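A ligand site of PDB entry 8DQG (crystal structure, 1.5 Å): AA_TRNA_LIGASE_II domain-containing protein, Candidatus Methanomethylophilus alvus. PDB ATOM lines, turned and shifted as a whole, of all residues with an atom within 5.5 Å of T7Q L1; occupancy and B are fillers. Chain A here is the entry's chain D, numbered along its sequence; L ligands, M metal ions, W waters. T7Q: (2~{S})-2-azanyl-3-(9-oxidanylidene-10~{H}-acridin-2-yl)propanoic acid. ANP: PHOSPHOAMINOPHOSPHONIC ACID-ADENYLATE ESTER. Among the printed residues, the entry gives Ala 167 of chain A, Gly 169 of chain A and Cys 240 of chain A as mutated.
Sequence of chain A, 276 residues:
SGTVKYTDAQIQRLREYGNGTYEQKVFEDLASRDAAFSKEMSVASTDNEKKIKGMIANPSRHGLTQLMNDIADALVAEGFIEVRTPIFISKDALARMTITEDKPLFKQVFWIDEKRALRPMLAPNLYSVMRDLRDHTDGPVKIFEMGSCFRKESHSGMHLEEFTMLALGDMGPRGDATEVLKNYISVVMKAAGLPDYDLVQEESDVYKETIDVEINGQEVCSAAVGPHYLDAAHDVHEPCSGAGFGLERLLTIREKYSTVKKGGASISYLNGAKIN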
ATOM      1  N   MET A  97      17.216  15.373 -21.189  1.00  0.00           N
ATOM      2  CA  MET A  97      17.976  16.317 -20.385  1.00  0.00           C
ATOM      3  C   MET A  97      17.113  16.995 -19.330  1.00  0.00           C
ATOM      4  O   MET A  97      17.618  17.898 -18.648  1.00  0.00           O
ATOM      5  CB  MET A  97      18.536  17.427 -21.280  1.00  0.00           C
ATOM      6  CG  MET A  97      19.632  16.999 -22.237  1.00  0.00           C
ATOM      7  SD  MET A  97      21.043  16.178 -21.491  1.00  0.00           S
ATOM      8  CE  MET A  97      21.656  17.424 -20.355  1.00  0.00           C
ATOM      9  N   PRO A 120      20.499  23.475 -28.097  1.00  0.00           N
ATOM     10  CA  PRO A 120      20.921  24.592 -27.238  1.00  0.00           C
ATOM     11  C   PRO A 120      22.143  24.271 -26.396  1.00  0.00           C
ATOM     12  O   PRO A 120      22.623  25.147 -25.656  1.00  0.00           O
ATOM     13  CB  PRO A 120      19.685  24.793 -26.334  1.00  0.00           C
ATOM     14  CG  PRO A 120      19.143  23.390 -26.186  1.00  0.00           C
ATOM     15  CD  PRO A 120      19.393  22.690 -27.502  1.00  0.00           C
ATOM     16  N   MET A 121      22.603  23.027 -26.446  1.00  0.00           N
ATOM     17  CA  MET A 121      23.741  22.518 -25.671  1.00  0.00           C
ATOM     18  C   MET A 121      24.229  21.282 -26.412  1.00  0.00           C
ATOM     19  O   MET A 121      23.514  20.706 -27.234  1.00  0.00           O
ATOM     20  CB  MET A 121      23.311  22.156 -24.248  1.00  0.00           C
ATOM     21  CG  MET A 121      22.023  21.226 -24.173  1.00  0.00           C
ATOM     22  SD  MET A 121      21.736  20.682 -22.531  1.00  0.00           S
ATOM     23  CE  MET A 121      21.362  22.200 -21.682  1.00  0.00           C
ATOM     24  N   LEU A 122      25.470  20.890 -26.127  1.00  0.00           N
ATOM     25  CA  LEU A 122      26.070  19.730 -26.758  1.00  0.00           C
ATOM     26  C   LEU A 122      25.813  18.428 -26.001  1.00  0.00           C
ATOM     27  O   LEU A 122      25.982  17.356 -26.587  1.00  0.00           O
ATOM     28  CB  LEU A 122      27.589  19.949 -26.886  1.00  0.00           C
ATOM     29  CG  LEU A 122      28.005  21.109 -27.821  1.00  0.00           C
ATOM     30  CD1 LEU A 122      29.513  21.225 -27.887  1.00  0.00           C
ATOM     31  CD2 LEU A 122      27.411  20.951 -29.237  1.00  0.00           C
ATOM     32  N   ALA A 123      25.408  18.505 -24.722  1.00  0.00           N
ATOM     33  CA  ALA A 123      25.315  17.311 -23.890  1.00  0.00           C
ATOM     34  C   ALA A 123      24.435  16.207 -24.480  1.00  0.00           C
ATOM     35  O   ALA A 123      24.800  15.032 -24.336  1.00  0.00           O
ATOM     36  CB  ALA A 123      24.836  17.681 -22.478  1.00  0.00           C
ATOM     37  N   LEU A 126      26.547  14.323 -26.944  1.00  0.00           N
ATOM     38  CA  LEU A 126      27.734  13.743 -26.315  1.00  0.00           C
ATOM     39  C   LEU A 126      27.377  12.585 -25.398  1.00  0.00           C
ATOM     40  O   LEU A 126      28.093  11.570 -25.371  1.00  0.00           O
ATOM     41  CB  LEU A 126      28.546  14.800 -25.560  1.00  0.00           C
ATOM     42  CG  LEU A 126      29.145  15.898 -26.435  1.00  0.00           C
ATOM     43  CD1 LEU A 126      29.978  16.867 -25.607  1.00  0.00           C
ATOM     44  CD2 LEU A 126      29.954  15.329 -27.593  1.00  0.00           C
ATOM     45  N   TYR A 127      26.288  12.685 -24.649  1.00  0.00           N
ATOM     46  CA  TYR A 127      25.849  11.529 -23.865  1.00  0.00           C
ATOM     47  C   TYR A 127      25.656  10.310 -24.755  1.00  0.00           C
ATOM     48  O   TYR A 127      26.026   9.178 -24.376  1.00  0.00           O
ATOM     49  CB  TYR A 127      24.549  11.804 -23.117  1.00  0.00           C
ATOM     50  CG  TYR A 127      24.644  12.216 -21.664  1.00  0.00           C
ATOM     51  CD1 TYR A 127      25.136  11.326 -20.710  1.00  0.00           C
ATOM     52  CD2 TYR A 127      24.081  13.408 -21.220  1.00  0.00           C
ATOM     53  CE1 TYR A 127      25.167  11.646 -19.357  1.00  0.00           C
ATOM     54  CE2 TYR A 127      24.081  13.735 -19.878  1.00  0.00           C
ATOM     55  CZ  TYR A 127      24.624  12.854 -18.951  1.00  0.00           C
ATOM     56  OH  TYR A 127      24.637  13.186 -17.628  1.00  0.00           O
ATOM     57  N   MET A 130      29.196   9.035 -26.011  1.00  0.00           N
ATOM     58  CA  MET A 130      29.950   8.443 -24.904  1.00  0.00           C
ATOM     59  C   MET A 130      29.403   7.068 -24.543  1.00  0.00           C
ATOM     60  O   MET A 130      30.176   6.129 -24.327  1.00  0.00           O
ATOM     61  CB  MET A 130      29.868   9.345 -23.677  1.00  0.00           C
ATOM     62  CG  MET A 130      30.842  10.471 -23.715  1.00  0.00           C
ATOM     63  SD  MET A 130      30.669  11.532 -22.296  1.00  0.00           S
ATOM     64  CE  MET A 130      30.422  10.335 -21.028  1.00  0.00           C
ATOM     65  N   ARG A 151      20.245  29.593 -28.789  1.00  0.00           N
ATOM     66  CA  ARG A 151      19.239  29.895 -27.770  1.00  0.00           C
ATOM     67  C   ARG A 151      18.623  31.260 -28.056  1.00  0.00           C
ATOM     68  O   ARG A 151      19.323  32.194 -28.439  1.00  0.00           O
ATOM     69  CB  ARG A 151      19.893  29.976 -26.378  1.00  0.00           C
ATOM     70  CG  ARG A 151      20.411  28.654 -25.851  1.00  0.00           C
ATOM     71  CD  ARG A 151      21.030  28.755 -24.469  1.00  0.00           C
ATOM     72  NE  ARG A 151      21.765  27.520 -24.188  1.00  0.00           N
ATOM     73  CZ  ARG A 151      22.311  27.211 -23.013  1.00  0.00           C
ATOM     74  NH1 ARG A 151      22.170  27.991 -21.959  1.00  0.00           N
ATOM     75  NH2 ARG A 151      23.029  26.096 -22.915  1.00  0.00           N
ATOM     76  N   MET A 165      30.044  26.380 -28.205  1.00  0.00           N
ATOM     77  CA  MET A 165      30.362  25.643 -26.992  1.00  0.00           C
ATOM     78  C   MET A 165      31.524  24.695 -27.258  1.00  0.00           C
ATOM     79  O   MET A 165      31.596  24.058 -28.313  1.00  0.00           O
ATOM     80  CB  MET A 165      29.142  24.841 -26.513  1.00  0.00           C
ATOM     81  CG  MET A 165      29.306  24.231 -25.123  1.00  0.00           C
ATOM     82  SD  MET A 165      27.812  23.445 -24.420  1.00  0.00           S
ATOM     83  CE  MET A 165      26.674  24.811 -24.440  1.00  0.00           C
ATOM     84  N   ALA A 167      32.347  21.376 -25.281  1.00  0.00           N
ATOM     85  CA  ALA A 167      31.848  20.493 -24.245  1.00  0.00           C
ATOM     86  C   ALA A 167      32.732  19.268 -24.211  1.00  0.00           C
ATOM     87  O   ALA A 167      33.122  18.727 -25.258  1.00  0.00           O
ATOM     88  CB  ALA A 167      30.391  20.090 -24.462  1.00  0.00           C
ATOM     89  N   LEU A 168      33.084  18.835 -23.002  1.00  0.00           N
ATOM     90  CA  LEU A 168      33.834  17.611 -22.810  1.00  0.00           C
ATOM     91  C   LEU A 168      33.081  16.687 -21.886  1.00  0.00           C
ATOM     92  O   LEU A 168      32.284  17.121 -21.060  1.00  0.00           O
ATOM     93  CB  LEU A 168      35.252  17.916 -22.302  1.00  0.00           C
ATOM     94  CG  LEU A 168      35.610  18.597 -20.999  1.00  0.00           C
ATOM     95  CD1 LEU A 168      35.462  17.623 -19.860  1.00  0.00           C
ATOM     96  CD2 LEU A 168      37.036  19.142 -21.103  1.00  0.00           C
ATOM     97  N   GLY A 169      33.292  15.391 -22.088  1.00  0.00           N
ATOM     98  CA  GLY A 169      32.727  14.376 -21.195  1.00  0.00           C
ATOM     99  C   GLY A 169      33.770  13.342 -20.859  1.00  0.00           C
ATOM    100  O   GLY A 169      34.604  13.014 -21.685  1.00  0.00           O
ATOM    101  N   TYR A 207      21.296  20.241 -13.686  1.00  0.00           N
ATOM    102  CA  TYR A 207      22.339  19.483 -13.005  1.00  0.00           C
ATOM    103  C   TYR A 207      22.273  19.564 -11.485  1.00  0.00           C
ATOM    104  O   TYR A 207      23.107  18.926 -10.820  1.00  0.00           O
ATOM    105  CB  TYR A 207      23.719  19.976 -13.476  1.00  0.00           C
ATOM    106  CG  TYR A 207      23.922  19.791 -14.961  1.00  0.00           C
ATOM    107  CD1 TYR A 207      24.320  18.572 -15.472  1.00  0.00           C
ATOM    108  CD2 TYR A 207      23.678  20.835 -15.855  1.00  0.00           C
ATOM    109  CE1 TYR A 207      24.498  18.400 -16.827  1.00  0.00           C
ATOM    110  CE2 TYR A 207      23.856  20.663 -17.209  1.00  0.00           C
ATOM    111  CZ  TYR A 207      24.267  19.446 -17.700  1.00  0.00           C
ATOM    112  OH  TYR A 207      24.431  19.270 -19.055  1.00  0.00           O
ATOM    113  N   THR A 210      26.254  22.992 -10.208  1.00  0.00           N
ATOM    114  CA  THR A 210      27.398  22.934 -11.103  1.00  0.00           C
ATOM    115  C   THR A 210      28.614  23.527 -10.395  1.00  0.00           C
ATOM    116  O   THR A 210      28.489  24.257  -9.394  1.00  0.00           O
ATOM    117  CB  THR A 210      27.138  23.717 -12.410  1.00  0.00           C
ATOM    118  OG1 THR A 210      26.756  25.053 -12.109  1.00  0.00           O
ATOM    119  CG2 THR A 210      26.048  23.046 -13.281  1.00  0.00           C
ATOM    120  N   SER A 222      30.254  25.968 -17.190  1.00  0.00           N
ATOM    121  CA  SER A 222      29.594  25.187 -16.151  1.00  0.00           C
ATOM    122  C   SER A 222      29.988  23.725 -16.291  1.00  0.00           C
ATOM    123  O   SER A 222      30.003  23.193 -17.399  1.00  0.00           O
ATOM    124  CB  SER A 222      28.076  25.243 -16.251  1.00  0.00           C
ATOM    125  OG  SER A 222      27.602  26.449 -15.743  1.00  0.00           O
ATOM    126  N   ALA A 223      30.255  23.083 -15.172  1.00  0.00           N
ATOM    127  CA  ALA A 223      30.675  21.684 -15.166  1.00  0.00           C
ATOM    128  C   ALA A 223      29.908  20.936 -14.086  1.00  0.00           C
ATOM    129  O   ALA A 223      29.455  21.530 -13.106  1.00  0.00           O
ATOM    130  CB  ALA A 223      32.187  21.572 -14.940  1.00  0.00           C
ATOM    131  N   ALA A 224      29.768  19.627 -14.260  1.00  0.00           N
ATOM    132  CA  ALA A 224      29.051  18.849 -13.271  1.00  0.00           C
ATOM    133  C   ALA A 224      29.457  17.385 -13.341  1.00  0.00           C
ATOM    134  O   ALA A 224      29.794  16.853 -14.410  1.00  0.00           O
ATOM    135  CB  ALA A 224      27.525  18.974 -13.437  1.00  0.00           C
ATOM    136  N   GLY A 226      27.640  14.067 -13.019  1.00  0.00           N
ATOM    137  CA  GLY A 226      26.249  13.634 -13.076  1.00  0.00           C
ATOM    138  C   GLY A 226      25.312  14.810 -13.247  1.00  0.00           C
ATOM    139  O   GLY A 226      25.538  15.689 -14.090  1.00  0.00           O
ATOM    140  N   CYS A 240      30.644   9.879 -13.912  1.00  0.00           N
ATOM    141  CA  CYS A 240      30.643  10.592 -15.167  1.00  0.00           C
ATOM    142  C   CYS A 240      30.724  12.057 -14.842  1.00  0.00           C
ATOM    143  O   CYS A 240      30.196  12.515 -13.806  1.00  0.00           O
ATOM    144  CB  CYS A 240      29.374  10.315 -15.971  1.00  0.00           C
ATOM    145  SG  CYS A 240      29.429  10.814 -17.705  1.00  0.00           S
ATOM    146  N   SER A 241      31.369  12.807 -15.724  1.00  0.00           N
ATOM    147  CA  SER A 241      31.439  14.237 -15.563  1.00  0.00           C
ATOM    148  C   SER A 241      31.542  14.892 -16.931  1.00  0.00           C
ATOM    149  O   SER A 241      31.801  14.261 -17.950  1.00  0.00           O
ATOM    150  CB  SER A 241      32.613  14.628 -14.672  1.00  0.00           C
ATOM    151  OG  SER A 241      33.790  14.665 -15.428  1.00  0.00           O
ATOM    152  N   GLY A 242      31.269  16.186 -16.941  1.00  0.00           N
ATOM    153  CA  GLY A 242      31.377  16.949 -18.160  1.00  0.00           C
ATOM    154  C   GLY A 242      31.427  18.422 -17.855  1.00  0.00           C
ATOM    155  O   GLY A 242      31.166  18.883 -16.740  1.00  0.00           O
ATOM    156  N   ALA A 243      31.728  19.175 -18.907  1.00  0.00           N
ATOM    157  CA  ALA A 243      31.853  20.623 -18.773  1.00  0.00           C
ATOM    158  C   ALA A 243      31.543  21.276 -20.113  1.00  0.00           C
ATOM    159  O   ALA A 243      31.825  20.729 -21.174  1.00  0.00           O
ATOM    160  CB  ALA A 243      33.283  20.974 -18.340  1.00  0.00           C
ATOM    161  N   GLY A 244      30.968  22.478 -20.040  1.00  0.00           N
ATOM    162  CA  GLY A 244      30.695  23.236 -21.250  1.00  0.00           C
ATOM    163  C   GLY A 244      31.200  24.665 -21.106  1.00  0.00           C
ATOM    164  O   GLY A 244      30.855  25.372 -20.134  1.00  0.00           O
HETATM  165  C10 T7Q L   1      27.899  18.736 -18.686  1.00  0.00           C
HETATM  166  C11 T7Q L   1      27.878  19.210 -19.972  1.00  0.00           C
HETATM  167  C12 T7Q L   1      27.775  20.568 -20.193  1.00  0.00           C
HETATM  168  C13 T7Q L   1      27.667  21.407 -19.112  1.00  0.00           C
HETATM  169  C14 T7Q L   1      27.683  20.945 -17.805  1.00  0.00           C
HETATM  170  C15 T7Q L   1      27.796  19.605 -17.592  1.00  0.00           C
HETATM  171  CB  T7Q L   1      27.521  22.897 -19.485  1.00  0.00           C
HETATM  172  CA  T7Q L   1      26.066  23.433 -19.553  1.00  0.00           C
HETATM  173  C   T7Q L   1      25.325  22.779 -20.714  1.00  0.00           C
HETATM  174  C02 T7Q L   1      27.985  18.290 -21.150  1.00  0.00           C
HETATM  175  C03 T7Q L   1      28.112  16.790 -20.910  1.00  0.00           C
HETATM  176  C04 T7Q L   1      28.225  15.899 -21.964  1.00  0.00           C
HETATM  177  C05 T7Q L   1      28.324  14.532 -21.744  1.00  0.00           C
HETATM  178  C06 T7Q L   1      28.334  14.041 -20.460  1.00  0.00           C
HETATM  179  C07 T7Q L   1      28.233  14.933 -19.374  1.00  0.00           C
HETATM  180  C08 T7Q L   1      28.127  16.306 -19.614  1.00  0.00           C
HETATM  181  N09 T7Q L   1      28.005  17.261 -18.454  1.00  0.00           N
HETATM  182  N   T7Q L   1      25.338  23.199 -18.309  1.00  0.00           N
HETATM  183  O01 T7Q L   1      28.131  18.791 -22.268  1.00  0.00           O
HETATM  184  O   T7Q L   1      24.933  23.522 -21.687  1.00  0.00           O
HETATM  185  OXT T7Q L   1      25.056  21.563 -20.743  1.00  0.00           O
HETATM  186  PG  ANP L   2      24.198  32.241 -18.402  1.00  0.00           P
HETATM  187  O1G ANP L   2      25.277  33.273 -18.546  1.00  0.00           O
HETATM  188  O2G ANP L   2      23.566  32.256 -16.954  1.00  0.00           O
HETATM  189  O3G ANP L   2      23.052  32.440 -19.484  1.00  0.00           O
HETATM  190  PB  ANP L   2      24.035  29.298 -18.683  1.00  0.00           P
HETATM  191  O1B ANP L   2      23.912  28.689 -17.311  1.00  0.00           O
HETATM  192  O2B ANP L   2      22.663  29.549 -19.355  1.00  0.00           O
HETATM  193  N3B ANP L   2      24.927  30.726 -18.628  1.00  0.00           N
HETATM  194  PA  ANP L   2      25.150  26.818 -19.710  1.00  0.00           P
HETATM  195  O1A ANP L   2      25.800  26.363 -18.464  1.00  0.00           O
HETATM  196  O2A ANP L   2      23.782  26.207 -20.082  1.00  0.00           O
HETATM  197  O3A ANP L   2      24.947  28.417 -19.593  1.00  0.00           O
HETATM  198  O5' ANP L   2      26.181  26.751 -20.920  1.00  0.00           O
HETATM  199  C5' ANP L   2      27.616  26.465 -20.821  1.00  0.00           C
HETATM  200  C4' ANP L   2      28.384  27.704 -21.177  1.00  0.00           C
HETATM  201  O4' ANP L   2      27.961  28.175 -22.475  1.00  0.00           O
HETATM  202  C3' ANP L   2      28.190  28.907 -20.259  1.00  0.00           C
HETATM  203  O3' ANP L   2      29.020  28.798 -19.109  1.00  0.00           O
HETATM  204  C2' ANP L   2      28.566  30.077 -21.174  1.00  0.00           C
HETATM  205  O2' ANP L   2      29.965  30.302 -21.154  1.00  0.00           O
HETATM  206  C1' ANP L   2      28.125  29.576 -22.554  1.00  0.00           C
HETATM  207  N9  ANP L   2      26.875  30.163 -23.014  1.00  0.00           N
HETATM  208  C8  ANP L   2      25.598  29.797 -22.661  1.00  0.00           C
HETATM  209  N7  ANP L   2      24.653  30.501 -23.252  1.00  0.00           N
HETATM  210  C5  ANP L   2      25.357  31.394 -24.041  1.00  0.00           C
HETATM  211  C6  ANP L   2      24.945  32.405 -24.932  1.00  0.00           C
HETATM  212  N6  ANP L   2      23.672  32.697 -25.187  1.00  0.00           N
HETATM  213  N1  ANP L   2      25.918  33.117 -25.547  1.00  0.00           N
HETATM  214  C2  ANP L   2      27.197  32.814 -25.324  1.00  0.00           C
HETATM  215  N3  ANP L   2      27.709  31.882 -24.513  1.00  0.00           N
HETATM  216  C4  ANP L   2      26.733  31.206 -23.905  1.00  0.00           C
HETATM  217 MG    MG M   1      25.824  27.761 -16.579  1.00  0.00          MG
HETATM  218  O   HOH W   1      27.544  15.931 -15.928  1.00  0.00           O
HETATM  219  O   HOH W   2      26.493  20.888 -23.216  1.00  0.00           O
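OH of Tyr 207 is in hydrogen-bond range of OXT of T7Q L1. The guanidinium group (NH2) of Arg 151 is in salt-bridge range of an oxygen (O) of T7Q L1, at 3.4 Å. NH2 of Arg 151 is in salt-bridge range of O2A of ANP L2.
An oxygen (O1A) of ANP L2 sits close to a nitrogen (N) of T7Q L1 (3.2 Å).
The guanidinium group of Arg 151 is in hydrogen-bond range of the backbone carbonyl oxygen of Pro 120. O of Ser 222 is in hydrogen-bond range of N of Gly 244, at 2.9 Å. The backbone carbonyl oxygen of Ala 243 sits at hydrogen-bond distance from the backbone NH of Leu 168 (2.9 Å). The backbone carbonyl oxygen (O) of Gly 242 sits at hydrogen-bond distance from the backbone NH (N) of Ala 224, at 2.9 Å.
Met 121 touches T7Q L1. Ala 123 touches T7Q L1 (CB to C02, 3.5 Å). Leu 126 touches T7Q L1. N of Tyr 127 touches C05 of T7Q L1 (3.999 Å). Met 130 touches T7Q L1. CE of Met 165 touches O of T7Q L1, 3.5 Å away. Ala 167 touches T7Q L1. Ser 222 touches T7Q L1. N of Ala 224 touches C15 of T7Q L1 (3.9 Å). Ser 241 touches T7Q L1. CA of Gly 242 touches N09 of T7Q L1 (3.4 Å). Ala 243 touches T7Q L1 (C to C12, 3.8 Å). Gly 244 touches T7Q L1 (N to CB, 3.5 Å). Hydrophobic or aromatic side chains that line T7Q L1: Met 121, Ala 123, Leu 126, Met 130, Met 165, Ala 167 and Tyr 207. 15 residues have an atom within 4 Å of T7Q L1: Met 121, Ala 123, Leu 126, Tyr 127, Met 130, Arg 151, Met 165, Ala 167, Tyr 207, Ser 222, Ala 224, Ser 241, Gly 242, Ala 243 and Gly 244. The nearest printed residue that does not touch T7Q L1 is Ala 223 (4.1 Å).
Water W2 lies within hydrogen-bond range of O01 of T7Q L1 (2.8 Å), N of Ala 123 (3.0 Å), N of Leu 122 (3.1 Å) and SD of Met 165 (3.1 Å). Water W1 lies within hydrogen-bond range of O of Gly 226 (2.7 Å), O of Ala 224 (2.9 Å) and N09 of T7Q L1 (2.9 Å).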
